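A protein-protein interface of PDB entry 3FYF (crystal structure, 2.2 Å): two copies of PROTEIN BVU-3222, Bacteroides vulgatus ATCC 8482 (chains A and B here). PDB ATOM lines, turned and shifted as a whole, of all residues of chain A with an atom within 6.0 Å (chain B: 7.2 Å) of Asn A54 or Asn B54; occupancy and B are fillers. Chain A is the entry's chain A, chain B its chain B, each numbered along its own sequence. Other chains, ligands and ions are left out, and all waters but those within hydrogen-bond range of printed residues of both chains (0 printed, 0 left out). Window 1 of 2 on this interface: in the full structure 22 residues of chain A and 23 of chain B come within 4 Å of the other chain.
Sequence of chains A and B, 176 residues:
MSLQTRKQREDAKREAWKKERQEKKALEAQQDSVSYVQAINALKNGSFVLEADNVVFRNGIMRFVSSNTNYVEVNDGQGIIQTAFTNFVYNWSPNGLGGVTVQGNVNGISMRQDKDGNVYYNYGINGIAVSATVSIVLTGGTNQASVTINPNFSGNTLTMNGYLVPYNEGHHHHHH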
ATOM      1  N   ALA A  52      -7.456  -9.166   9.113  1.00  0.00           N
ATOM      2  CA  ALA A  52      -6.466  -8.298   9.755  1.00  0.00           C
ATOM      3  C   ALA A  52      -7.049  -7.424  10.869  1.00  0.00           C
ATOM      4  O   ALA A  52      -8.022  -6.696  10.666  1.00  0.00           O
ATOM      5  CB  ALA A  52      -5.752  -7.426   8.718  1.00  0.00           C
ATOM      6  N   ASP A  53      -6.441  -7.521  12.046  1.00  0.00           N
ATOM      7  CA  ASP A  53      -6.684  -6.584  13.122  1.00  0.00           C
ATOM      8  C   ASP A  53      -5.786  -5.362  12.960  1.00  0.00           C
ATOM      9  O   ASP A  53      -6.216  -4.231  13.166  1.00  0.00           O
ATOM     10  CB  ASP A  53      -6.407  -7.236  14.471  1.00  0.00           C
ATOM     11  CG  ASP A  53      -6.598  -6.273  15.617  1.00  0.00           C
ATOM     12  OD1 ASP A  53      -7.714  -5.732  15.737  1.00  0.00           O
ATOM     13  OD2 ASP A  53      -5.630  -6.035  16.372  1.00  0.00           O
ATOM     14  N   ASN A  54      -4.527  -5.600  12.602  1.00  0.00           N
ATOM     15  CA  ASN A  54      -3.605  -4.500  12.331  1.00  0.00           C
ATOM     16  C   ASN A  54      -2.691  -4.777  11.157  1.00  0.00           C
ATOM     17  O   ASN A  54      -2.480  -5.924  10.779  1.00  0.00           O
ATOM     18  CB  ASN A  54      -2.779  -4.140  13.573  1.00  0.00           C
ATOM     19  CG  ASN A  54      -2.010  -5.311  14.119  1.00  0.00           C
ATOM     20  OD1 ASN A  54      -2.520  -6.083  14.938  1.00  0.00           O
ATOM     21  ND2 ASN A  54      -0.764  -5.441  13.691  1.00  0.00           N
ATOM     22  N   VAL A  55      -2.169  -3.699  10.582  1.00  0.00           N
ATOM     23  CA  VAL A  55      -1.298  -3.752   9.417  1.00  0.00           C
ATOM     24  C   VAL A  55       0.036  -3.075   9.763  1.00  0.00           C
ATOM     25  O   VAL A  55       0.029  -1.997  10.356  1.00  0.00           O
ATOM     26  CB  VAL A  55      -1.979  -3.052   8.196  1.00  0.00           C
ATOM     27  CG1 VAL A  55      -1.079  -3.042   6.997  1.00  0.00           C
ATOM     28  CG2 VAL A  55      -3.294  -3.732   7.836  1.00  0.00           C
ATOM     29  N   VAL A  56       1.156  -3.704   9.396  1.00  0.00           N
ATOM     30  CA  VAL A  56       2.492  -3.130   9.601  1.00  0.00           C
ATOM     31  C   VAL A  56       3.127  -2.890   8.241  1.00  0.00           C
ATOM     32  O   VAL A  56       3.216  -3.801   7.423  1.00  0.00           O
ATOM     33  CB  VAL A  56       3.405  -4.039  10.486  1.00  0.00           C
ATOM     34  CG1 VAL A  56       4.848  -3.483  10.596  1.00  0.00           C
ATOM     35  CG2 VAL A  56       2.810  -4.194  11.870  1.00  0.00           C
ATOM     36  N   MET A  62       2.550   0.982  12.012  1.00  0.00           N
ATOM     37  CA  MET A  62       1.430   0.076  12.203  1.00  0.00           C
ATOM     38  C   MET A  62       0.127   0.824  12.456  1.00  0.00           C
ATOM     39  O   MET A  62       0.094   1.856  13.134  1.00  0.00           O
ATOM     40  CB  MET A  62       1.704  -1.081  13.195  1.00  0.00           C
ATOM     41  CG  MET A  62       1.186  -0.966  14.607  1.00  0.00           C
ATOM     42  SD  MET A  62      -0.566  -1.212  15.016  1.00  0.00           S
ATOM     43  CE  MET A  62      -0.453  -0.100  16.382  1.00  0.00           C
ATOM     44  N   ARG A  63      -0.940   0.279  11.886  1.00  0.00           N
ATOM     45  CA  ARG A  63      -2.254   0.858  12.012  1.00  0.00           C
ATOM     46  C   ARG A  63      -3.256  -0.238  12.338  1.00  0.00           C
ATOM     47  O   ARG A  63      -3.299  -1.256  11.653  1.00  0.00           O
ATOM     48  CB  ARG A  63      -2.626   1.530  10.691  1.00  0.00           C
ATOM     49  CG  ARG A  63      -3.135   2.945  10.842  1.00  0.00           C
ATOM     50  CD  ARG A  63      -4.533   2.997  11.363  1.00  0.00           C
ATOM     51  NE  ARG A  63      -5.058   4.355  11.389  1.00  0.00           N
ATOM     52  CZ  ARG A  63      -6.099   4.726  12.123  1.00  0.00           C
ATOM     53  NH1 ARG A  63      -6.707   3.843  12.908  1.00  0.00           N
ATOM     54  NH2 ARG A  63      -6.525   5.980  12.080  1.00  0.00           N
ATOM     55  N   PHE A  64      -4.056  -0.036  13.384  1.00  0.00           N
ATOM     56  CA  PHE A  64      -5.173  -0.945  13.676  1.00  0.00           C
ATOM     57  C   PHE A  64      -6.288  -0.678  12.671  1.00  0.00           C
ATOM     58  O   PHE A  64      -6.588   0.470  12.384  1.00  0.00           O
ATOM     59  CB  PHE A  64      -5.684  -0.753  15.104  1.00  0.00           C
ATOM     60  CG  PHE A  64      -4.761  -1.293  16.158  1.00  0.00           C
ATOM     61  CD1 PHE A  64      -4.547  -2.657  16.276  1.00  0.00           C
ATOM     62  CD2 PHE A  64      -4.114  -0.437  17.036  1.00  0.00           C
ATOM     63  CE1 PHE A  64      -3.693  -3.158  17.239  1.00  0.00           C
ATOM     64  CE2 PHE A  64      -3.275  -0.934  18.016  1.00  0.00           C
ATOM     65  CZ  PHE A  64      -3.059  -2.297  18.117  1.00  0.00           C
ATOM     66  N   VAL A  65      -6.865  -1.737  12.106  1.00  0.00           N
ATOM     67  CA  VAL A  65      -7.799  -1.594  10.982  1.00  0.00           C
ATOM     68  C   VAL A  65      -9.051  -2.443  11.164  1.00  0.00           C
ATOM     69  O   VAL A  65      -9.142  -3.240  12.102  1.00  0.00           O
ATOM     70  CB  VAL A  65      -7.142  -1.959   9.600  1.00  0.00           C
ATOM     71  CG1 VAL A  65      -5.935  -1.058   9.288  1.00  0.00           C
ATOM     72  CG2 VAL A  65      -6.749  -3.430   9.543  1.00  0.00           C
ATOM     73  N   THR A 159       2.594  -6.398   6.351  1.00  0.00           N
ATOM     74  CA  THR A 159       2.237  -7.516   7.209  1.00  0.00           C
ATOM     75  C   THR A 159       0.865  -7.273   7.836  1.00  0.00           C
ATOM     76  O   THR A 159       0.581  -6.170   8.274  1.00  0.00           O
ATOM     77  CB  THR A 159       3.327  -7.790   8.287  1.00  0.00           C
ATOM     78  OG1 THR A 159       4.573  -8.067   7.634  1.00  0.00           O
ATOM     79  CG2 THR A 159       2.963  -8.990   9.152  1.00  0.00           C
ATOM     80  N   MET A 160       0.022  -8.303   7.838  1.00  0.00           N
ATOM     81  CA  MET A 160      -1.299  -8.262   8.456  1.00  0.00           C
ATOM     82  C   MET A 160      -1.301  -9.194   9.652  1.00  0.00           C
ATOM     83  O   MET A 160      -0.918 -10.358   9.529  1.00  0.00           O
ATOM     84  CB  MET A 160      -2.376  -8.755   7.476  1.00  0.00           C
ATOM     85  CG  MET A 160      -2.575  -7.920   6.226  1.00  0.00           C
ATOM     86  SD  MET A 160      -4.140  -8.256   5.346  1.00  0.00           S
ATOM     87  CE  MET A 160      -4.057  -6.950   4.141  1.00  0.00           C
ATOM     88  N   ASN A 161      -1.741  -8.689  10.804  1.00  0.00           N
ATOM     89  CA  ASN A 161      -1.833  -9.509  12.009  1.00  0.00           C
ATOM     90  C   ASN A 161      -3.284  -9.632  12.427  1.00  0.00           C
ATOM     91  O   ASN A 161      -3.984  -8.627  12.540  1.00  0.00           O
ATOM     92  CB  ASN A 161      -1.019  -8.894  13.153  1.00  0.00           C
ATOM     93  CG  ASN A 161       0.464  -8.796  12.833  1.00  0.00           C
ATOM     94  OD1 ASN A 161       1.075  -7.731  12.947  1.00  0.00           O
ATOM     95  ND2 ASN A 161       1.042  -9.900  12.424  1.00  0.00           N
ATOM     96  N   GLY A 162      -3.731 -10.860  12.652  1.00  0.00           N
ATOM     97  CA  GLY A 162      -5.113 -11.099  13.024  1.00  0.00           C
ATOM     98  C   GLY A 162      -5.411 -12.565  13.218  1.00  0.00           C
ATOM     99  O   GLY A 162      -4.566 -13.319  13.694  1.00  0.00           O
ATOM    100  N   LEU B  50       4.288   2.658  26.121  1.00  0.00           N
ATOM    101  CA  LEU B  50       3.579   1.966  25.061  1.00  0.00           C
ATOM    102  C   LEU B  50       2.945   0.712  25.635  1.00  0.00           C
ATOM    103  O   LEU B  50       3.640  -0.202  26.064  1.00  0.00           O
ATOM    104  CB  LEU B  50       4.472   1.630  23.862  1.00  0.00           C
ATOM    105  CG  LEU B  50       3.607   1.030  22.735  1.00  0.00           C
ATOM    106  CD1 LEU B  50       3.790   1.785  21.456  1.00  0.00           C
ATOM    107  CD2 LEU B  50       3.778  -0.482  22.523  1.00  0.00           C
ATOM    108  N   GLU B  51       1.619   0.692  25.618  1.00  0.00           N
ATOM    109  CA  GLU B  51       0.831  -0.428  26.109  1.00  0.00           C
ATOM    110  C   GLU B  51       0.623  -1.426  24.969  1.00  0.00           C
ATOM    111  O   GLU B  51      -0.163  -1.166  24.054  1.00  0.00           O
ATOM    112  CB  GLU B  51      -0.516   0.096  26.614  1.00  0.00           C
ATOM    113  CG  GLU B  51      -0.417   1.146  27.735  1.00  0.00           C
ATOM    114  CD  GLU B  51      -1.765   1.703  28.154  1.00  0.00           C
ATOM    115  OE1 GLU B  51      -1.872   2.213  29.290  1.00  0.00           O
ATOM    116  OE2 GLU B  51      -2.720   1.642  27.346  1.00  0.00           O
ATOM    117  N   ALA B  52       1.327  -2.557  25.025  1.00  0.00           N
ATOM    118  CA  ALA B  52       1.334  -3.518  23.923  1.00  0.00           C
ATOM    119  C   ALA B  52       0.027  -4.286  23.783  1.00  0.00           C
ATOM    120  O   ALA B  52      -0.477  -4.895  24.745  1.00  0.00           O
ATOM    121  CB  ALA B  52       2.487  -4.489  24.057  1.00  0.00           C
ATOM    122  N   ASP B  53      -0.510  -4.236  22.567  1.00  0.00           N
ATOM    123  CA  ASP B  53      -1.643  -5.043  22.161  1.00  0.00           C
ATOM    124  C   ASP B  53      -1.168  -6.380  21.585  1.00  0.00           C
ATOM    125  O   ASP B  53      -1.739  -7.432  21.882  1.00  0.00           O
ATOM    126  CB  ASP B  53      -2.463  -4.289  21.125  1.00  0.00           C
ATOM    127  CG  ASP B  53      -3.570  -5.131  20.546  1.00  0.00           C
ATOM    128  OD1 ASP B  53      -4.530  -5.442  21.287  1.00  0.00           O
ATOM    129  OD2 ASP B  53      -3.473  -5.488  19.354  1.00  0.00           O
ATOM    130  N   ASN B  54      -0.128  -6.338  20.754  1.00  0.00           N
ATOM    131  CA  ASN B  54       0.480  -7.567  20.253  1.00  0.00           C
ATOM    132  C   ASN B  54       2.001  -7.486  20.158  1.00  0.00           C
ATOM    133  O   ASN B  54       2.573  -6.408  20.188  1.00  0.00           O
ATOM    134  CB  ASN B  54      -0.131  -7.989  18.905  1.00  0.00           C
ATOM    135  CG  ASN B  54       0.098  -6.975  17.815  1.00  0.00           C
ATOM    136  OD1 ASN B  54       1.122  -7.001  17.126  1.00  0.00           O
ATOM    137  ND2 ASN B  54      -0.864  -6.084  17.633  1.00  0.00           N
ATOM    138  N   VAL B  55       2.636  -8.644  20.035  1.00  0.00           N
ATOM    139  CA  VAL B  55       4.081  -8.739  19.983  1.00  0.00           C
ATOM    140  C   VAL B  55       4.431  -9.612  18.792  1.00  0.00           C
ATOM    141  O   VAL B  55       3.785 -10.631  18.582  1.00  0.00           O
ATOM    142  CB  VAL B  55       4.664  -9.316  21.319  1.00  0.00           C
ATOM    143  CG1 VAL B  55       6.107  -9.724  21.168  1.00  0.00           C
ATOM    144  CG2 VAL B  55       4.515  -8.295  22.457  1.00  0.00           C
ATOM    145  N   VAL B  56       5.415  -9.172  18.001  1.00  0.00           N
ATOM    146  CA  VAL B  56       5.921  -9.911  16.834  1.00  0.00           C
ATOM    147  C   VAL B  56       7.399 -10.266  17.048  1.00  0.00           C
ATOM    148  O   VAL B  56       8.217  -9.402  17.355  1.00  0.00           O
ATOM    149  CB  VAL B  56       5.729  -9.110  15.495  1.00  0.00           C
ATOM    150  CG1 VAL B  56       6.173  -9.928  14.286  1.00  0.00           C
ATOM    151  CG2 VAL B  56       4.270  -8.681  15.320  1.00  0.00           C
ATOM    152  N   MET B  62       3.379 -13.870  15.750  1.00  0.00           N
ATOM    153  CA  MET B  62       2.697 -12.797  16.460  1.00  0.00           C
ATOM    154  C   MET B  62       1.677 -13.346  17.453  1.00  0.00           C
ATOM    155  O   MET B  62       0.962 -14.305  17.161  1.00  0.00           O
ATOM    156  CB  MET B  62       2.011 -11.852  15.471  1.00  0.00           C
ATOM    157  CG  MET B  62       0.537 -12.147  15.250  1.00  0.00           C
ATOM    158  SD  MET B  62      -0.529 -11.286  16.423  1.00  0.00           S
ATOM    159  CE  MET B  62      -2.097 -12.094  16.111  1.00  0.00           C
ATOM    160  N   ARG B  63       1.619 -12.728  18.627  1.00  0.00           N
ATOM    161  CA  ARG B  63       0.666 -13.095  19.651  1.00  0.00           C
ATOM    162  C   ARG B  63      -0.003 -11.844  20.191  1.00  0.00           C
ATOM    163  O   ARG B  63       0.674 -10.852  20.475  1.00  0.00           O
ATOM    164  CB  ARG B  63       1.367 -13.845  20.781  1.00  0.00           C
ATOM    165  CG  ARG B  63       0.700 -15.158  21.149  1.00  0.00           C
ATOM    166  CD  ARG B  63      -0.246 -15.009  22.309  1.00  0.00           C
ATOM    167  NE  ARG B  63      -0.840 -16.287  22.689  1.00  0.00           N
ATOM    168  CZ  ARG B  63      -2.030 -16.409  23.266  1.00  0.00           C
ATOM    169  NH1 ARG B  63      -2.489 -17.610  23.584  1.00  0.00           N
ATOM    170  NH2 ARG B  63      -2.765 -15.330  23.518  1.00  0.00           N
ATOM    171  N   PHE B  64      -1.329 -11.888  20.308  1.00  0.00           N
ATOM    172  CA  PHE B  64      -2.075 -10.839  21.011  1.00  0.00           C
ATOM    173  C   PHE B  64      -1.853 -10.985  22.503  1.00  0.00           C
ATOM    174  O   PHE B  64      -1.692 -12.091  23.017  1.00  0.00           O
ATOM    175  CB  PHE B  64      -3.567 -10.856  20.659  1.00  0.00           C
ATOM    176  CG  PHE B  64      -3.856 -10.277  19.317  1.00  0.00           C
ATOM    177  CD1 PHE B  64      -3.695  -8.917  19.091  1.00  0.00           C
ATOM    178  CD2 PHE B  64      -4.231 -11.085  18.263  1.00  0.00           C
ATOM    179  CE1 PHE B  64      -3.927  -8.378  17.847  1.00  0.00           C
ATOM    180  CE2 PHE B  64      -4.472 -10.541  17.011  1.00  0.00           C
ATOM    181  CZ  PHE B  64      -4.314  -9.188  16.806  1.00  0.00           C
ATOM    182  N   VAL B  65      -1.841  -9.854  23.197  1.00  0.00           N
ATOM    183  CA  VAL B  65      -1.193  -9.796  24.489  1.00  0.00           C
ATOM    184  C   VAL B  65      -1.860  -8.793  25.435  1.00  0.00           C
ATOM    185  O   VAL B  65      -2.570  -7.891  24.990  1.00  0.00           O
ATOM    186  CB  VAL B  65       0.334  -9.546  24.247  1.00  0.00           C
ATOM    187  CG1 VAL B  65       0.835  -8.224  24.825  1.00  0.00           C
ATOM    188  CG2 VAL B  65       1.156 -10.753  24.650  1.00  0.00           C
ATOM    189  N   SER B  66      -1.674  -8.985  26.739  1.00  0.00           N
ATOM    190  CA  SER B  66      -2.114  -7.994  27.721  1.00  0.00           C
ATOM    191  C   SER B  66      -1.036  -6.937  27.944  1.00  0.00           C
ATOM    192  O   SER B  66       0.137  -7.263  28.088  1.00  0.00           O
ATOM    193  CB  SER B  66      -2.476  -8.659  29.050  1.00  0.00           C
ATOM    194  OG  SER B  66      -2.618  -7.683  30.073  1.00  0.00           O
ATOM    195  N   ASN B  70       3.238  -6.561  29.179  1.00  0.00           N
ATOM    196  CA  ASN B  70       4.073  -6.235  28.020  1.00  0.00           C
ATOM    197  C   ASN B  70       3.983  -4.747  27.733  1.00  0.00           C
ATOM    198  O   ASN B  70       2.970  -4.256  27.237  1.00  0.00           O
ATOM    199  CB  ASN B  70       3.678  -7.034  26.772  1.00  0.00           C
ATOM    200  CG  ASN B  70       3.771  -8.536  26.975  1.00  0.00           C
ATOM    201  OD1 ASN B  70       4.769  -9.160  26.615  1.00  0.00           O
ATOM    202  ND2 ASN B  70       2.724  -9.124  27.554  1.00  0.00           N
ATOM    203  N   GLN B 144      -1.366   5.187  17.918  1.00  0.00           N
ATOM    204  CA  GLN B 144      -0.991   3.829  17.565  1.00  0.00           C
ATOM    205  C   GLN B 144       0.486   3.806  17.198  1.00  0.00           C
ATOM    206  O   GLN B 144       0.950   4.582  16.360  1.00  0.00           O
ATOM    207  CB  GLN B 144      -1.874   3.325  16.427  1.00  0.00           C
ATOM    208  CG  GLN B 144      -3.334   3.231  16.836  1.00  0.00           C
ATOM    209  CD  GLN B 144      -4.266   3.050  15.666  1.00  0.00           C
ATOM    210  OE1 GLN B 144      -3.885   2.504  14.629  1.00  0.00           O
ATOM    211  NE2 GLN B 144      -5.507   3.503  15.829  1.00  0.00           N
ATOM    212  N   LEU B 158      12.395  -8.229  18.761  1.00  0.00           N
ATOM    213  CA  LEU B 158      11.029  -8.144  19.275  1.00  0.00           C
ATOM    214  C   LEU B 158      10.360  -6.805  18.961  1.00  0.00           C
ATOM    215  O   LEU B 158      10.919  -5.746  19.216  1.00  0.00           O
ATOM    216  CB  LEU B 158      11.020  -8.416  20.791  1.00  0.00           C
ATOM    217  CG  LEU B 158       9.676  -8.608  21.502  1.00  0.00           C
ATOM    218  CD1 LEU B 158       9.729  -9.748  22.506  1.00  0.00           C
ATOM    219  CD2 LEU B 158       9.218  -7.329  22.170  1.00  0.00           C
ATOM    220  N   THR B 159       9.146  -6.870  18.424  1.00  0.00           N
ATOM    221  CA  THR B 159       8.367  -5.673  18.145  1.00  0.00           C
ATOM    222  C   THR B 159       7.064  -5.706  18.954  1.00  0.00           C
ATOM    223  O   THR B 159       6.388  -6.722  18.971  1.00  0.00           O
ATOM    224  CB  THR B 159       8.062  -5.552  16.635  1.00  0.00           C
ATOM    225  OG1 THR B 159       9.291  -5.540  15.895  1.00  0.00           O
ATOM    226  CG2 THR B 159       7.295  -4.278  16.328  1.00  0.00           C
ATOM    227  N   MET B 160       6.740  -4.604  19.631  1.00  0.00           N
ATOM    228  CA  MET B 160       5.462  -4.437  20.333  1.00  0.00           C
ATOM    229  C   MET B 160       4.603  -3.425  19.598  1.00  0.00           C
ATOM    230  O   MET B 160       5.040  -2.296  19.357  1.00  0.00           O
ATOM    231  CB  MET B 160       5.673  -3.911  21.758  1.00  0.00           C
ATOM    232  CG  MET B 160       6.440  -4.829  22.687  1.00  0.00           C
ATOM    233  SD  MET B 160       6.378  -4.317  24.425  1.00  0.00           S
ATOM    234  CE  MET B 160       7.207  -5.724  25.084  1.00  0.00           C
ATOM    235  N   ASN B 161       3.378  -3.827  19.260  1.00  0.00           N
ATOM    236  CA  ASN B 161       2.422  -2.941  18.605  1.00  0.00           C
ATOM    237  C   ASN B 161       1.306  -2.619  19.560  1.00  0.00           C
ATOM    238  O   ASN B 161       0.697  -3.518  20.116  1.00  0.00           O
ATOM    239  CB  ASN B 161       1.849  -3.597  17.345  1.00  0.00           C
ATOM    240  CG  ASN B 161       2.923  -3.904  16.320  1.00  0.00           C
ATOM    241  OD1 ASN B 161       3.630  -3.005  15.867  1.00  0.00           O
ATOM    242  ND2 ASN B 161       3.053  -5.174  15.955  1.00  0.00           N
ATOM    243  N   GLY B 162       1.032  -1.335  19.747  1.00  0.00           N
ATOM    244  CA  GLY B 162       0.009  -0.935  20.702  1.00  0.00           C
ATOM    245  C   GLY B 162      -0.246   0.550  20.736  1.00  0.00           C
ATOM    246  O   GLY B 162      -0.155   1.225  19.713  1.00  0.00           O
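Among the printed residues, merely in contact across the chains: Phe A64 with Asp B53, Asp A53 with Phe B64, Met A62 with Asn B161, Met A62 with Gly B162, Asn A161 with Met B62, Gly A162 with Met B62, Met A62 with Gln B144, Asp A53 with Asp B53 and Asn A54 with Phe B64.
Hydrophobic or aromatic side chains of chain A within 4 Å of the printed part of chain B: Met A62 and Phe A64.
Among the printed residues, 12 pairs touch across the chains.
Among the printed residues, no Asp or Glu carboxylate lies within 4 Å of a Lys or Arg side-chain nitrogen of the other chain.
Of the printed residues of chain B, Met A62 touches Gln B144 (3.7 Å), Asn B161 (3.4 Å) and Gly B162 (3.6 Å).
Of the printed residues of chain B, Asn A161 touches Met B62 (3.6 Å).
The nearest residue of chain A that does not touch Asn B54 is Phe A64 (4.1 Å).
The side-chain amide oxygen (OD1) of Asn A54 lies within hydrogen-bond range of the side-chain amide nitrogen (ND2) of Asn B54.
The guanidinium group of Arg A63 sits close to the side-chain amide nitrogen of Gln B144.
N of Phe A64 sits at hydrogen-bond distance from OE1 of Gln B144 (2.8 Å).
OD2 of Asp A53 sits close to OD1 of Asn A54.
The backbone carbonyl oxygen (O) of Asp A53 lies within hydrogen-bond range of the backbone NH (N) of Val A65, at 2.8 Å.
The backbone NH of Asn A161 is in hydrogen-bond range of the backbone carbonyl oxygen of Asn A54 (2.9 Å).
The backbone NH of Val A55 sits at hydrogen-bond distance from the backbone carbonyl oxygen of Arg A63, 2.9 Å away.
The side-chain amide nitrogen (ND2) of Asn B54 lies within hydrogen-bond range of the side-chain carboxylate (OD2) of Asp B53, 3.2 Å away.
O of Asp B53 lies within hydrogen-bond range of N of Val B65 (2.8 Å).
Asp A53 touches its own counterpart, Asp B53.
Asn A54 touches its own counterpart, Asn B54.
Asn A54 touches Phe B64, but with the chains exchanged Phe A64 does not touch Asn B54 (4.1 Å).
Met A62 touches Asn B161, and with the chains exchanged Asn A161 touches Met B62.
Positions printed for both chains: 52, 53, 54, 55, 56, 62, 63, 64, 65, 159, 160, 161 and 162.
Of the 12 pairs that touch across the chains among the printed residues, 8 have their exchanged pair printed and touching as well.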
